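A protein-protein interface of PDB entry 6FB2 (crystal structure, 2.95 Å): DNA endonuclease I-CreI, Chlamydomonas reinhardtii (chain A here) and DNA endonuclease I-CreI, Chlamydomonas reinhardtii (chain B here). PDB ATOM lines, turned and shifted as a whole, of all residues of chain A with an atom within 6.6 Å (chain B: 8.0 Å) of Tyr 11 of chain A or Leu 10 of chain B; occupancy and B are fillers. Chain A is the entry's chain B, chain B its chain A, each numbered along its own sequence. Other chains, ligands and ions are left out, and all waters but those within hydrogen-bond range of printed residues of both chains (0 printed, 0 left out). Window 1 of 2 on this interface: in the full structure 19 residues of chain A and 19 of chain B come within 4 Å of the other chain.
Of chain B, only Leu 10, Ala 13, Gly 14, Asp 17, Phe 93 and Lys 95 come within 4 Å of Tyr 11 of chain A.
Printed residues of chain A within 4 Å of Leu 10 of chain B: Glu 7, Leu 10 and Tyr 11.
Of the printed residues of chain A, Leu 96 of chain B touches Phe 15 (3.97 Å) and Phe 53 (3.6 Å).
Printed residues of chain A within 4 Å of Tyr 11 of chain B: Leu 10, Ala 13 and Gly 14.
Of the printed residues of chain A, Asp 17 of chain B touches Tyr 11 (2.3 Å) and Phe 15 (3.6 Å).
Printed residues of chain B within 4 Å of Leu 10 of chain A: Glu 7 (3.7 Å), Leu 10 (3.8 Å) and Tyr 11 (3.3 Å).
Of the printed residues of chain A, Ala 13 of chain B touches Tyr 11 (3.7 Å).
Phe 8 of chain B touches none of the printed residues of chain A.
The nearest residue of chain B that does not touch Tyr 11 of chain A is Tyr 11 of chain B (4.3 Å).
The nearest printed residue of chain B that does not touch Leu 10 of chain A is Leu 12 of chain B (5.6 Å).
Among the printed residues, pairs that only touch across the chains: Glu 7 of chain A with Leu 10 of chain B (3.8 Å), Leu 10 of chain A with Glu 7 of chain B (3.7 Å), Leu 10 of chain A with Leu 10 of chain B (3.8 Å), Leu 10 of chain A with Tyr 11 of chain B (3.3 Å), Tyr 11 of chain A with Leu 10 of chain B (3.4 Å), Tyr 11 of chain A with Ala 13 of chain B (3.7 Å), Tyr 11 of chain A with Gly 14 of chain B (3.4 Å), Tyr 11 of chain A with Phe 93 of chain B (3.3 Å), Tyr 11 of chain A with Lys 95 of chain B (3.3 Å), Ala 13 of chain A with Tyr 11 of chain B (3.9 Å), Gly 14 of chain A with Tyr 11 of chain B (3.4 Å), Gly 14 of chain A with Gly 14 of chain B (3.6 Å), Gly 14 of chain A with Phe 15 of chain B (3.3 Å), Gly 14 of chain A with Ser 18 of chain B (3.95 Å), Phe 15 of chain A with Gly 14 of chain B (3.1 Å), Phe 15 of chain A with Phe 15 of chain B (3.9 Å), Phe 15 of chain A with Asp 17 of chain B (3.6 Å), Phe 15 of chain A with Ser 18 of chain B (3.7 Å), Phe 15 of chain A with Leu 96 of chain B (3.97 Å) and Phe 53 of chain A with Leu 96 of chain B (3.6 Å).
The side-chain amide oxygen (OD1) of Asn 5 of chain B lies within hydrogen-bond range of the backbone NH (N) of Glu 7 of chain B (3.1 Å).
The side-chain hydroxyl (OG) of Ser 18 of chain B sits at hydrogen-bond distance from the backbone carbonyl oxygen (O) of Gly 14 of chain B.
The backbone carbonyl oxygen of Phe 15 of chain B sits at hydrogen-bond distance from the side-chain hydroxyl of Ser 18 of chain B (2.6 Å).
The side-chain carboxylate of Asp 17 of chain B lies within hydrogen-bond range of the backbone NH of Lys 95 of chain B (2.8 Å).
N of Leu 96 of chain B is in hydrogen-bond range of OD2 of Asp 17 of chain B, 3.3 Å away.
OD1 of Asp 17 of chain B is in hydrogen-bond range of N of Lys 97 of chain B (3.0 Å).
Hydrophobic or aromatic side chains of chain A within 4 Å of the printed part of chain B: Leu 10, Tyr 11, Phe 15 and Phe 53.
Among the printed residues, 23 pairs touch across the chains.
The side-chain amino group (NZ) of Lys 6 of chain B is in salt-bridge range of the side-chain carboxylate (OE2) of Glu 7 of chain A (2.4 Å).
OE2 of Glu 7 of chain B lies within salt-bridge range of NZ of Lys 6 of chain A (3.2 Å).
OD2 of Asp 17 of chain B sits close to OH of Tyr 11 of chain A (2.3 Å).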
ATOM      1  N   LYS A   6      13.689 -30.789  -5.444  1.00  0.00           N
ATOM      2  CA  LYS A   6      12.883 -29.647  -5.029  1.00  0.00           C
ATOM      3  C   LYS A   6      12.725 -28.642  -6.164  1.00  0.00           C
ATOM      4  O   LYS A   6      11.715 -27.946  -6.247  1.00  0.00           O
ATOM      5  CB  LYS A   6      13.493 -28.972  -3.800  1.00  0.00           C
ATOM      6  CG  LYS A   6      12.547 -28.016  -3.091  1.00  0.00           C
ATOM      7  CD  LYS A   6      13.161 -27.493  -1.804  1.00  0.00           C
ATOM      8  CE  LYS A   6      12.183 -26.608  -1.047  1.00  0.00           C
ATOM      9  NZ  LYS A   6      12.770 -26.096   0.223  1.00  0.00           N
ATOM     10  N   GLU A   7      13.725 -28.572  -7.039  1.00  0.00           N
ATOM     11  CA  GLU A   7      13.649 -27.703  -8.208  1.00  0.00           C
ATOM     12  C   GLU A   7      12.660 -28.257  -9.230  1.00  0.00           C
ATOM     13  O   GLU A   7      12.041 -27.505  -9.983  1.00  0.00           O
ATOM     14  CB  GLU A   7      15.026 -27.536  -8.853  1.00  0.00           C
ATOM     15  CG  GLU A   7      16.058 -26.853  -7.969  1.00  0.00           C
ATOM     16  CD  GLU A   7      17.249 -26.340  -8.759  1.00  0.00           C
ATOM     17  OE1 GLU A   7      17.135 -26.217  -9.997  1.00  0.00           O
ATOM     18  OE2 GLU A   7      18.299 -26.060  -8.143  1.00  0.00           O
ATOM     19  N   PHE A   8      12.520 -29.578  -9.253  1.00  0.00           N
ATOM     20  CA  PHE A   8      11.577 -30.235 -10.147  1.00  0.00           C
ATOM     21  C   PHE A   8      10.151 -30.058  -9.644  1.00  0.00           C
ATOM     22  O   PHE A   8       9.250 -29.728 -10.413  1.00  0.00           O
ATOM     23  CB  PHE A   8      11.909 -31.720 -10.274  1.00  0.00           C
ATOM     24  CG  PHE A   8      10.872 -32.510 -11.015  1.00  0.00           C
ATOM     25  CD1 PHE A   8      10.687 -32.330 -12.377  1.00  0.00           C
ATOM     26  CD2 PHE A   8      10.088 -33.439 -10.352  1.00  0.00           C
ATOM     27  CE1 PHE A   8       9.732 -33.059 -13.061  1.00  0.00           C
ATOM     28  CE2 PHE A   8       9.135 -34.172 -11.032  1.00  0.00           C
ATOM     29  CZ  PHE A   8       8.957 -33.982 -12.387  1.00  0.00           C
ATOM     30  N   LEU A   9       9.954 -30.275  -8.348  1.00  0.00           N
ATOM     31  CA  LEU A   9       8.631 -30.157  -7.748  1.00  0.00           C
ATOM     32  C   LEU A   9       8.152 -28.708  -7.697  1.00  0.00           C
ATOM     33  O   LEU A   9       6.951 -28.449  -7.711  1.00  0.00           O
ATOM     34  CB  LEU A   9       8.616 -30.771  -6.348  1.00  0.00           C
ATOM     35  CG  LEU A   9       8.824 -32.285  -6.284  1.00  0.00           C
ATOM     36  CD1 LEU A   9       8.766 -32.774  -4.853  1.00  0.00           C
ATOM     37  CD2 LEU A   9       7.792 -32.998  -7.132  1.00  0.00           C
ATOM     38  N   LEU A  10       9.093 -27.770  -7.637  1.00  0.00           N
ATOM     39  CA  LEU A  10       8.751 -26.351  -7.622  1.00  0.00           C
ATOM     40  C   LEU A  10       8.212 -25.887  -8.971  1.00  0.00           C
ATOM     41  O   LEU A  10       7.157 -25.256  -9.038  1.00  0.00           O
ATOM     42  CB  LEU A  10       9.957 -25.507  -7.208  1.00  0.00           C
ATOM     43  CG  LEU A  10      10.050 -25.209  -5.711  1.00  0.00           C
ATOM     44  CD1 LEU A  10      11.388 -24.598  -5.348  1.00  0.00           C
ATOM     45  CD2 LEU A  10       8.926 -24.280  -5.309  1.00  0.00           C
ATOM     46  N   TYR A  11       8.940 -26.201 -10.038  1.00  0.00           N
ATOM     47  CA  TYR A  11       8.511 -25.854 -11.386  1.00  0.00           C
ATOM     48  C   TYR A  11       7.184 -26.524 -11.713  1.00  0.00           C
ATOM     49  O   TYR A  11       6.219 -25.856 -12.086  1.00  0.00           O
ATOM     50  CB  TYR A  11       9.569 -26.272 -12.410  1.00  0.00           C
ATOM     51  CG  TYR A  11       9.171 -26.012 -13.848  1.00  0.00           C
ATOM     52  CD1 TYR A  11       8.487 -26.970 -14.586  1.00  0.00           C
ATOM     53  CD2 TYR A  11       9.482 -24.812 -14.467  1.00  0.00           C
ATOM     54  CE1 TYR A  11       8.119 -26.735 -15.892  1.00  0.00           C
ATOM     55  CE2 TYR A  11       9.123 -24.572 -15.776  1.00  0.00           C
ATOM     56  CZ  TYR A  11       8.440 -25.536 -16.482  1.00  0.00           C
ATOM     57  OH  TYR A  11       8.076 -25.301 -17.784  1.00  0.00           O
ATOM     58  N   LEU A  12       7.153 -27.846 -11.570  1.00  0.00           N
ATOM     59  CA  LEU A  12       5.984 -28.642 -11.923  1.00  0.00           C
ATOM     60  C   LEU A  12       4.721 -28.177 -11.197  1.00  0.00           C
ATOM     61  O   LEU A  12       3.657 -28.080 -11.805  1.00  0.00           O
ATOM     62  CB  LEU A  12       6.251 -30.124 -11.648  1.00  0.00           C
ATOM     63  CG  LEU A  12       5.257 -31.127 -12.236  1.00  0.00           C
ATOM     64  CD1 LEU A  12       5.113 -30.921 -13.730  1.00  0.00           C
ATOM     65  CD2 LEU A  12       5.693 -32.550 -11.938  1.00  0.00           C
ATOM     66  N   ALA A  13       4.845 -27.878  -9.908  1.00  0.00           N
ATOM     67  CA  ALA A  13       3.707 -27.402  -9.124  1.00  0.00           C
ATOM     68  C   ALA A  13       3.111 -26.141  -9.735  1.00  0.00           C
ATOM     69  O   ALA A  13       1.888 -25.990  -9.803  1.00  0.00           O
ATOM     70  CB  ALA A  13       4.115 -27.149  -7.689  1.00  0.00           C
ATOM     71  N   GLY A  14       3.982 -25.238 -10.176  1.00  0.00           N
ATOM     72  CA  GLY A  14       3.544 -24.045 -10.874  1.00  0.00           C
ATOM     73  C   GLY A  14       2.857 -24.398 -12.176  1.00  0.00           C
ATOM     74  O   GLY A  14       1.880 -23.759 -12.563  1.00  0.00           O
ATOM     75  N   PHE A  15       3.367 -25.427 -12.847  1.00  0.00           N
ATOM     76  CA  PHE A  15       2.791 -25.880 -14.107  1.00  0.00           C
ATOM     77  C   PHE A  15       1.482 -26.635 -13.872  1.00  0.00           C
ATOM     78  O   PHE A  15       0.599 -26.636 -14.729  1.00  0.00           O
ATOM     79  CB  PHE A  15       3.787 -26.759 -14.866  1.00  0.00           C
ATOM     80  CG  PHE A  15       3.499 -26.875 -16.337  1.00  0.00           C
ATOM     81  CD1 PHE A  15       4.046 -25.971 -17.236  1.00  0.00           C
ATOM     82  CD2 PHE A  15       2.692 -27.890 -16.825  1.00  0.00           C
ATOM     83  CE1 PHE A  15       3.787 -26.073 -18.589  1.00  0.00           C
ATOM     84  CE2 PHE A  15       2.430 -27.997 -18.179  1.00  0.00           C
ATOM     85  CZ  PHE A  15       2.978 -27.087 -19.059  1.00  0.00           C
ATOM     86  N   VAL A  16       1.361 -27.274 -12.710  1.00  0.00           N
ATOM     87  CA  VAL A  16       0.129 -27.972 -12.347  1.00  0.00           C
ATOM     88  C   VAL A  16      -0.985 -26.973 -12.034  1.00  0.00           C
ATOM     89  O   VAL A  16      -2.121 -27.130 -12.489  1.00  0.00           O
ATOM     90  CB  VAL A  16       0.344 -28.922 -11.149  1.00  0.00           C
ATOM     91  CG1 VAL A  16      -0.986 -29.446 -10.630  1.00  0.00           C
ATOM     92  CG2 VAL A  16       1.240 -30.079 -11.546  1.00  0.00           C
ATOM     93  N   PHE A  53       7.131 -32.779 -23.840  1.00  0.00           N
ATOM     94  CA  PHE A  53       7.136 -32.230 -22.493  1.00  0.00           C
ATOM     95  C   PHE A  53       6.412 -33.174 -21.541  1.00  0.00           C
ATOM     96  O   PHE A  53       6.800 -33.319 -20.382  1.00  0.00           O
ATOM     97  CB  PHE A  53       6.462 -30.857 -22.489  1.00  0.00           C
ATOM     98  CG  PHE A  53       6.537 -30.141 -21.170  1.00  0.00           C
ATOM     99  CD1 PHE A  53       7.655 -29.396 -20.834  1.00  0.00           C
ATOM    100  CD2 PHE A  53       5.479 -30.194 -20.275  1.00  0.00           C
ATOM    101  CE1 PHE A  53       7.724 -28.729 -19.628  1.00  0.00           C
ATOM    102  CE2 PHE A  53       5.544 -29.528 -19.066  1.00  0.00           C
ATOM    103  CZ  PHE A  53       6.668 -28.797 -18.743  1.00  0.00           C
ATOM    104  N   ASN B   5      14.165 -14.184  -5.639  1.00  0.00           N
ATOM    105  CA  ASN B   5      14.559 -15.473  -5.076  1.00  0.00           C
ATOM    106  C   ASN B   5      14.386 -16.626  -6.062  1.00  0.00           C
ATOM    107  O   ASN B   5      13.455 -16.630  -6.866  1.00  0.00           O
ATOM    108  CB  ASN B   5      13.779 -15.745  -3.786  1.00  0.00           C
ATOM    109  CG  ASN B   5      13.376 -17.204  -3.636  1.00  0.00           C
ATOM    110  OD1 ASN B   5      12.279 -17.600  -4.031  1.00  0.00           O
ATOM    111  ND2 ASN B   5      14.258 -18.008  -3.054  1.00  0.00           N
ATOM    112  N   LYS B   6      15.291 -17.598  -5.988  1.00  0.00           N
ATOM    113  CA  LYS B   6      15.310 -18.726  -6.913  1.00  0.00           C
ATOM    114  C   LYS B   6      14.037 -19.572  -6.862  1.00  0.00           C
ATOM    115  O   LYS B   6      13.509 -19.967  -7.903  1.00  0.00           O
ATOM    116  CB  LYS B   6      16.531 -19.604  -6.638  1.00  0.00           C
ATOM    117  CG  LYS B   6      16.666 -20.794  -7.575  1.00  0.00           C
ATOM    118  CD  LYS B   6      17.856 -21.659  -7.193  1.00  0.00           C
ATOM    119  CE  LYS B   6      17.970 -22.866  -8.107  1.00  0.00           C
ATOM    120  NZ  LYS B   6      19.031 -23.815  -7.662  1.00  0.00           N
ATOM    121  N   GLU B   7      13.552 -19.850  -5.655  1.00  0.00           N
ATOM    122  CA  GLU B   7      12.355 -20.672  -5.491  1.00  0.00           C
ATOM    123  C   GLU B   7      11.107 -19.983  -6.035  1.00  0.00           C
ATOM    124  O   GLU B   7      10.199 -20.641  -6.541  1.00  0.00           O
ATOM    125  CB  GLU B   7      12.149 -21.051  -4.024  1.00  0.00           C
ATOM    126  CG  GLU B   7      13.207 -21.990  -3.469  1.00  0.00           C
ATOM    127  CD  GLU B   7      12.702 -22.799  -2.291  1.00  0.00           C
ATOM    128  OE1 GLU B   7      11.548 -22.577  -1.865  1.00  0.00           O
ATOM    129  OE2 GLU B   7      13.456 -23.662  -1.795  1.00  0.00           O
ATOM    130  N   PHE B   8      11.064 -18.660  -5.924  1.00  0.00           N
ATOM    131  CA  PHE B   8       9.964 -17.883  -6.479  1.00  0.00           C
ATOM    132  C   PHE B   8       9.979 -17.941  -8.001  1.00  0.00           C
ATOM    133  O   PHE B   8       8.931 -18.037  -8.639  1.00  0.00           O
ATOM    134  CB  PHE B   8      10.044 -16.432  -6.005  1.00  0.00           C
ATOM    135  CG  PHE B   8       9.215 -15.481  -6.818  1.00  0.00           C
ATOM    136  CD1 PHE B   8       7.840 -15.427  -6.661  1.00  0.00           C
ATOM    137  CD2 PHE B   8       9.816 -14.631  -7.735  1.00  0.00           C
ATOM    138  CE1 PHE B   8       7.080 -14.548  -7.408  1.00  0.00           C
ATOM    139  CE2 PHE B   8       9.061 -13.752  -8.483  1.00  0.00           C
ATOM    140  CZ  PHE B   8       7.692 -13.709  -8.319  1.00  0.00           C
ATOM    141  N   LEU B   9      11.175 -17.880  -8.577  1.00  0.00           N
ATOM    142  CA  LEU B   9      11.336 -17.950 -10.023  1.00  0.00           C
ATOM    143  C   LEU B   9      10.992 -19.341 -10.553  1.00  0.00           C
ATOM    144  O   LEU B   9      10.417 -19.477 -11.634  1.00  0.00           O
ATOM    145  CB  LEU B   9      12.768 -17.575 -10.410  1.00  0.00           C
ATOM    146  CG  LEU B   9      13.186 -16.131 -10.125  1.00  0.00           C
ATOM    147  CD1 LEU B   9      14.684 -15.949 -10.289  1.00  0.00           C
ATOM    148  CD2 LEU B   9      12.436 -15.174 -11.031  1.00  0.00           C
ATOM    149  N   LEU B  10      11.345 -20.367  -9.782  1.00  0.00           N
ATOM    150  CA  LEU B  10      11.088 -21.754 -10.160  1.00  0.00           C
ATOM    151  C   LEU B  10       9.599 -22.054 -10.310  1.00  0.00           C
ATOM    152  O   LEU B  10       9.165 -22.531 -11.357  1.00  0.00           O
ATOM    153  CB  LEU B  10      11.718 -22.711  -9.146  1.00  0.00           C
ATOM    154  CG  LEU B  10      13.207 -23.004  -9.323  1.00  0.00           C
ATOM    155  CD1 LEU B  10      13.734 -23.847  -8.178  1.00  0.00           C
ATOM    156  CD2 LEU B  10      13.440 -23.709 -10.644  1.00  0.00           C
ATOM    157  N   TYR B  11       8.825 -21.782  -9.263  1.00  0.00           N
ATOM    158  CA  TYR B  11       7.381 -21.978  -9.317  1.00  0.00           C
ATOM    159  C   TYR B  11       6.767 -21.158 -10.443  1.00  0.00           C
ATOM    160  O   TYR B  11       5.988 -21.675 -11.243  1.00  0.00           O
ATOM    161  CB  TYR B  11       6.726 -21.588  -7.988  1.00  0.00           C
ATOM    162  CG  TYR B  11       5.211 -21.602  -8.031  1.00  0.00           C
ATOM    163  CD1 TYR B  11       4.493 -20.477  -8.422  1.00  0.00           C
ATOM    164  CD2 TYR B  11       4.499 -22.740  -7.682  1.00  0.00           C
ATOM    165  CE1 TYR B  11       3.120 -20.489  -8.472  1.00  0.00           C
ATOM    166  CE2 TYR B  11       3.119 -22.758  -7.723  1.00  0.00           C
ATOM    167  CZ  TYR B  11       2.438 -21.630  -8.121  1.00  0.00           C
ATOM    168  OH  TYR B  11       1.066 -21.637  -8.168  1.00  0.00           O
ATOM    169  N   LEU B  12       7.116 -19.875 -10.484  1.00  0.00           N
ATOM    170  CA  LEU B  12       6.529 -18.943 -11.439  1.00  0.00           C
ATOM    171  C   LEU B  12       6.801 -19.349 -12.885  1.00  0.00           C
ATOM    172  O   LEU B  12       5.924 -19.232 -13.739  1.00  0.00           O
ATOM    173  CB  LEU B  12       7.041 -17.524 -11.184  1.00  0.00           C
ATOM    174  CG  LEU B  12       6.508 -16.429 -12.107  1.00  0.00           C
ATOM    175  CD1 LEU B  12       5.002 -16.324 -11.988  1.00  0.00           C
ATOM    176  CD2 LEU B  12       7.156 -15.096 -11.794  1.00  0.00           C
ATOM    177  N   ALA B  13       8.014 -19.825 -13.150  1.00  0.00           N
ATOM    178  CA  ALA B  13       8.388 -20.268 -14.489  1.00  0.00           C
ATOM    179  C   ALA B  13       7.450 -21.358 -14.989  1.00  0.00           C
ATOM    180  O   ALA B  13       7.028 -21.342 -16.148  1.00  0.00           O
ATOM    181  CB  ALA B  13       9.818 -20.764 -14.500  1.00  0.00           C
ATOM    182  N   GLY B  14       7.129 -22.303 -14.111  1.00  0.00           N
ATOM    183  CA  GLY B  14       6.195 -23.360 -14.443  1.00  0.00           C
ATOM    184  C   GLY B  14       4.809 -22.821 -14.729  1.00  0.00           C
ATOM    185  O   GLY B  14       4.112 -23.319 -15.612  1.00  0.00           O
ATOM    186  N   PHE B  15       4.409 -21.796 -13.983  1.00  0.00           N
ATOM    187  CA  PHE B  15       3.104 -21.182 -14.176  1.00  0.00           C
ATOM    188  C   PHE B  15       3.057 -20.428 -15.501  1.00  0.00           C
ATOM    189  O   PHE B  15       2.043 -20.446 -16.199  1.00  0.00           O
ATOM    190  CB  PHE B  15       2.787 -20.236 -13.018  1.00  0.00           C
ATOM    191  CG  PHE B  15       1.324 -19.933 -12.864  1.00  0.00           C
ATOM    192  CD1 PHE B  15       0.709 -18.980 -13.660  1.00  0.00           C
ATOM    193  CD2 PHE B  15       0.565 -20.597 -11.915  1.00  0.00           C
ATOM    194  CE1 PHE B  15      -0.637 -18.704 -13.516  1.00  0.00           C
ATOM    195  CE2 PHE B  15      -0.778 -20.323 -11.768  1.00  0.00           C
ATOM    196  CZ  PHE B  15      -1.379 -19.376 -12.570  1.00  0.00           C
ATOM    197  N   VAL B  16       4.161 -19.769 -15.843  1.00  0.00           N
ATOM    198  CA  VAL B  16       4.248 -18.994 -17.078  1.00  0.00           C
ATOM    199  C   VAL B  16       4.248 -19.902 -18.309  1.00  0.00           C
ATOM    200  O   VAL B  16       3.585 -19.611 -19.305  1.00  0.00           O
ATOM    201  CB  VAL B  16       5.495 -18.082 -17.077  1.00  0.00           C
ATOM    202  CG1 VAL B  16       5.714 -17.454 -18.444  1.00  0.00           C
ATOM    203  CG2 VAL B  16       5.360 -17.003 -16.017  1.00  0.00           C
ATOM    204  N   ASP B  17       4.983 -21.009 -18.231  1.00  0.00           N
ATOM    205  CA  ASP B  17       5.036 -21.972 -19.328  1.00  0.00           C
ATOM    206  C   ASP B  17       3.667 -22.590 -19.602  1.00  0.00           C
ATOM    207  O   ASP B  17       3.414 -23.102 -20.692  1.00  0.00           O
ATOM    208  CB  ASP B  17       6.049 -23.080 -19.026  1.00  0.00           C
ATOM    209  CG  ASP B  17       7.474 -22.676 -19.351  1.00  0.00           C
ATOM    210  OD1 ASP B  17       7.660 -21.743 -20.157  1.00  0.00           O
ATOM    211  OD2 ASP B  17       8.409 -23.301 -18.809  1.00  0.00           O
ATOM    212  N   SER B  18       2.787 -22.535 -18.608  1.00  0.00           N
ATOM    213  CA  SER B  18       1.458 -23.123 -18.726  1.00  0.00           C
ATOM    214  C   SER B  18       0.398 -22.104 -19.145  1.00  0.00           C
ATOM    215  O   SER B  18      -0.142 -22.177 -20.247  1.00  0.00           O
ATOM    216  CB  SER B  18       1.056 -23.773 -17.404  1.00  0.00           C
ATOM    217  OG  SER B  18       1.154 -22.846 -16.337  1.00  0.00           O
ATOM    218  N   GLN B  89      16.073 -12.833 -15.098  1.00  0.00           N
ATOM    219  CA  GLN B  89      16.135 -13.707 -13.931  1.00  0.00           C
ATOM    220  C   GLN B  89      15.234 -14.935 -14.070  1.00  0.00           C
ATOM    221  O   GLN B  89      15.493 -15.970 -13.456  1.00  0.00           O
ATOM    222  CB  GLN B  89      15.773 -12.936 -12.656  1.00  0.00           C
ATOM    223  CG  GLN B  89      16.635 -11.710 -12.396  1.00  0.00           C
ATOM    224  CD  GLN B  89      16.588 -11.262 -10.947  1.00  0.00           C
ATOM    225  OE1 GLN B  89      16.694 -12.078 -10.031  1.00  0.00           O
ATOM    226  NE2 GLN B  89      16.434  -9.962 -10.733  1.00  0.00           N
ATOM    227  N   LEU B  90      14.181 -14.818 -14.876  1.00  0.00           N
ATOM    228  CA  LEU B  90      13.229 -15.912 -15.060  1.00  0.00           C
ATOM    229  C   LEU B  90      13.672 -16.884 -16.151  1.00  0.00           C
ATOM    230  O   LEU B  90      13.386 -18.079 -16.081  1.00  0.00           O
ATOM    231  CB  LEU B  90      11.841 -15.361 -15.395  1.00  0.00           C
ATOM    232  CG  LEU B  90      10.723 -16.396 -15.548  1.00  0.00           C
ATOM    233  CD1 LEU B  90      10.336 -16.977 -14.200  1.00  0.00           C
ATOM    234  CD2 LEU B  90       9.512 -15.801 -16.243  1.00  0.00           C
ATOM    235  N   PRO B  92      16.350 -18.685 -17.184  1.00  0.00           N
ATOM    236  CA  PRO B  92      16.995 -20.001 -17.068  1.00  0.00           C
ATOM    237  C   PRO B  92      16.057 -21.129 -16.634  1.00  0.00           C
ATOM    238  O   PRO B  92      16.415 -22.298 -16.782  1.00  0.00           O
ATOM    239  CB  PRO B  92      18.055 -19.772 -15.983  1.00  0.00           C
ATOM    240  CG  PRO B  92      18.292 -18.307 -15.978  1.00  0.00           C
ATOM    241  CD  PRO B  92      16.967 -17.698 -16.280  1.00  0.00           C
ATOM    242  N   PHE B  93      14.879 -20.789 -16.120  1.00  0.00           N
ATOM    243  CA  PHE B  93      13.965 -21.797 -15.592  1.00  0.00           C
ATOM    244  C   PHE B  93      12.805 -22.099 -16.537  1.00  0.00           C
ATOM    245  O   PHE B  93      12.049 -23.047 -16.319  1.00  0.00           O
ATOM    246  CB  PHE B  93      13.444 -21.368 -14.221  1.00  0.00           C
ATOM    247  CG  PHE B  93      14.521 -20.889 -13.295  1.00  0.00           C
ATOM    248  CD1 PHE B  93      15.436 -21.778 -12.759  1.00  0.00           C
ATOM    249  CD2 PHE B  93      14.620 -19.549 -12.963  1.00  0.00           C
ATOM    250  CE1 PHE B  93      16.430 -21.339 -11.907  1.00  0.00           C
ATOM    251  CE2 PHE B  93      15.610 -19.105 -12.113  1.00  0.00           C
ATOM    252  CZ  PHE B  93      16.516 -20.001 -11.584  1.00  0.00           C
ATOM    253  N   LEU B  94      12.667 -21.292 -17.583  1.00  0.00           N
ATOM    254  CA  LEU B  94      11.655 -21.540 -18.605  1.00  0.00           C
ATOM    255  C   LEU B  94      12.016 -22.772 -19.429  1.00  0.00           C
ATOM    256  O   LEU B  94      13.169 -22.950 -19.824  1.00  0.00           O
ATOM    257  CB  LEU B  94      11.501 -20.326 -19.520  1.00  0.00           C
ATOM    258  CG  LEU B  94      10.857 -19.088 -18.896  1.00  0.00           C
ATOM    259  CD1 LEU B  94      10.752 -17.965 -19.905  1.00  0.00           C
ATOM    260  CD2 LEU B  94       9.489 -19.428 -18.344  1.00  0.00           C
ATOM    261  N   LYS B  95      11.025 -23.620 -19.683  1.00  0.00           N
ATOM    262  CA  LYS B  95      11.243 -24.850 -20.436  1.00  0.00           C
ATOM    263  C   LYS B  95      10.558 -24.799 -21.798  1.00  0.00           C
ATOM    264  O   LYS B  95      11.091 -25.299 -22.790  1.00  0.00           O
ATOM    265  CB  LYS B  95      10.748 -26.061 -19.643  1.00  0.00           C
ATOM    266  CG  LYS B  95      11.530 -26.338 -18.367  1.00  0.00           C
ATOM    267  CD  LYS B  95      11.097 -27.651 -17.731  1.00  0.00           C
ATOM    268  CE  LYS B  95      12.013 -28.039 -16.582  1.00  0.00           C
ATOM    269  NZ  LYS B  95      11.735 -29.420 -16.094  1.00  0.00           N
ATOM    270  N   LEU B  96       9.378 -24.191 -21.840  1.00  0.00           N
ATOM    271  CA  LEU B  96       8.615 -24.102 -23.080  1.00  0.00           C
ATOM    272  C   LEU B  96       8.818 -22.759 -23.774  1.00  0.00           C
ATOM    273  O   LEU B  96       9.074 -22.706 -24.976  1.00  0.00           O
ATOM    274  CB  LEU B  96       7.125 -24.331 -22.817  1.00  0.00           C
ATOM    275  CG  LEU B  96       6.728 -25.727 -22.334  1.00  0.00           C
ATOM    276  CD1 LEU B  96       5.218 -25.889 -22.289  1.00  0.00           C
ATOM    277  CD2 LEU B  96       7.347 -26.784 -23.225  1.00  0.00           C
ATOM    278  N   LYS B  97       8.710 -21.678 -23.008  1.00  0.00           N
ATOM    279  CA  LYS B  97       8.770 -20.336 -23.573  1.00  0.00           C
ATOM    280  C   LYS B  97      10.121 -19.661 -23.352  1.00  0.00           C
ATOM    281  O   LYS B  97      10.200 -18.435 -23.293  1.00  0.00           O
ATOM    282  CB  LYS B  97       7.651 -19.468 -22.990  1.00  0.00           C
ATOM    283  CG  LYS B  97       6.262 -20.069 -23.143  1.00  0.00           C
ATOM    284  CD  LYS B  97       5.196 -19.200 -22.495  1.00  0.00           C
ATOM    285  CE  LYS B  97       3.851 -19.912 -22.463  1.00  0.00           C
ATOM    286  NZ  LYS B  97       3.315 -20.178 -23.822  1.00  0.00           N
ATOM    287  N   GLN B  98      11.181 -20.456 -23.240  1.00  0.00           N
ATOM    288  CA  GLN B  98      12.513 -19.904 -23.016  1.00  0.00           C
ATOM    289  C   GLN B  98      13.016 -19.130 -24.233  1.00  0.00           C
ATOM    290  O   GLN B  98      13.563 -18.036 -24.091  1.00  0.00           O
ATOM    291  CB  GLN B  98      13.508 -21.002 -22.632  1.00  0.00           C
ATOM    292  CG  GLN B  98      14.887 -20.470 -22.259  1.00  0.00           C
ATOM    293  CD  GLN B  98      15.836 -21.554 -21.789  1.00  0.00           C
ATOM    294  OE1 GLN B  98      15.957 -21.815 -20.593  1.00  0.00           O
ATOM    295  NE2 GLN B  98      16.524 -22.187 -22.730  1.00  0.00           N
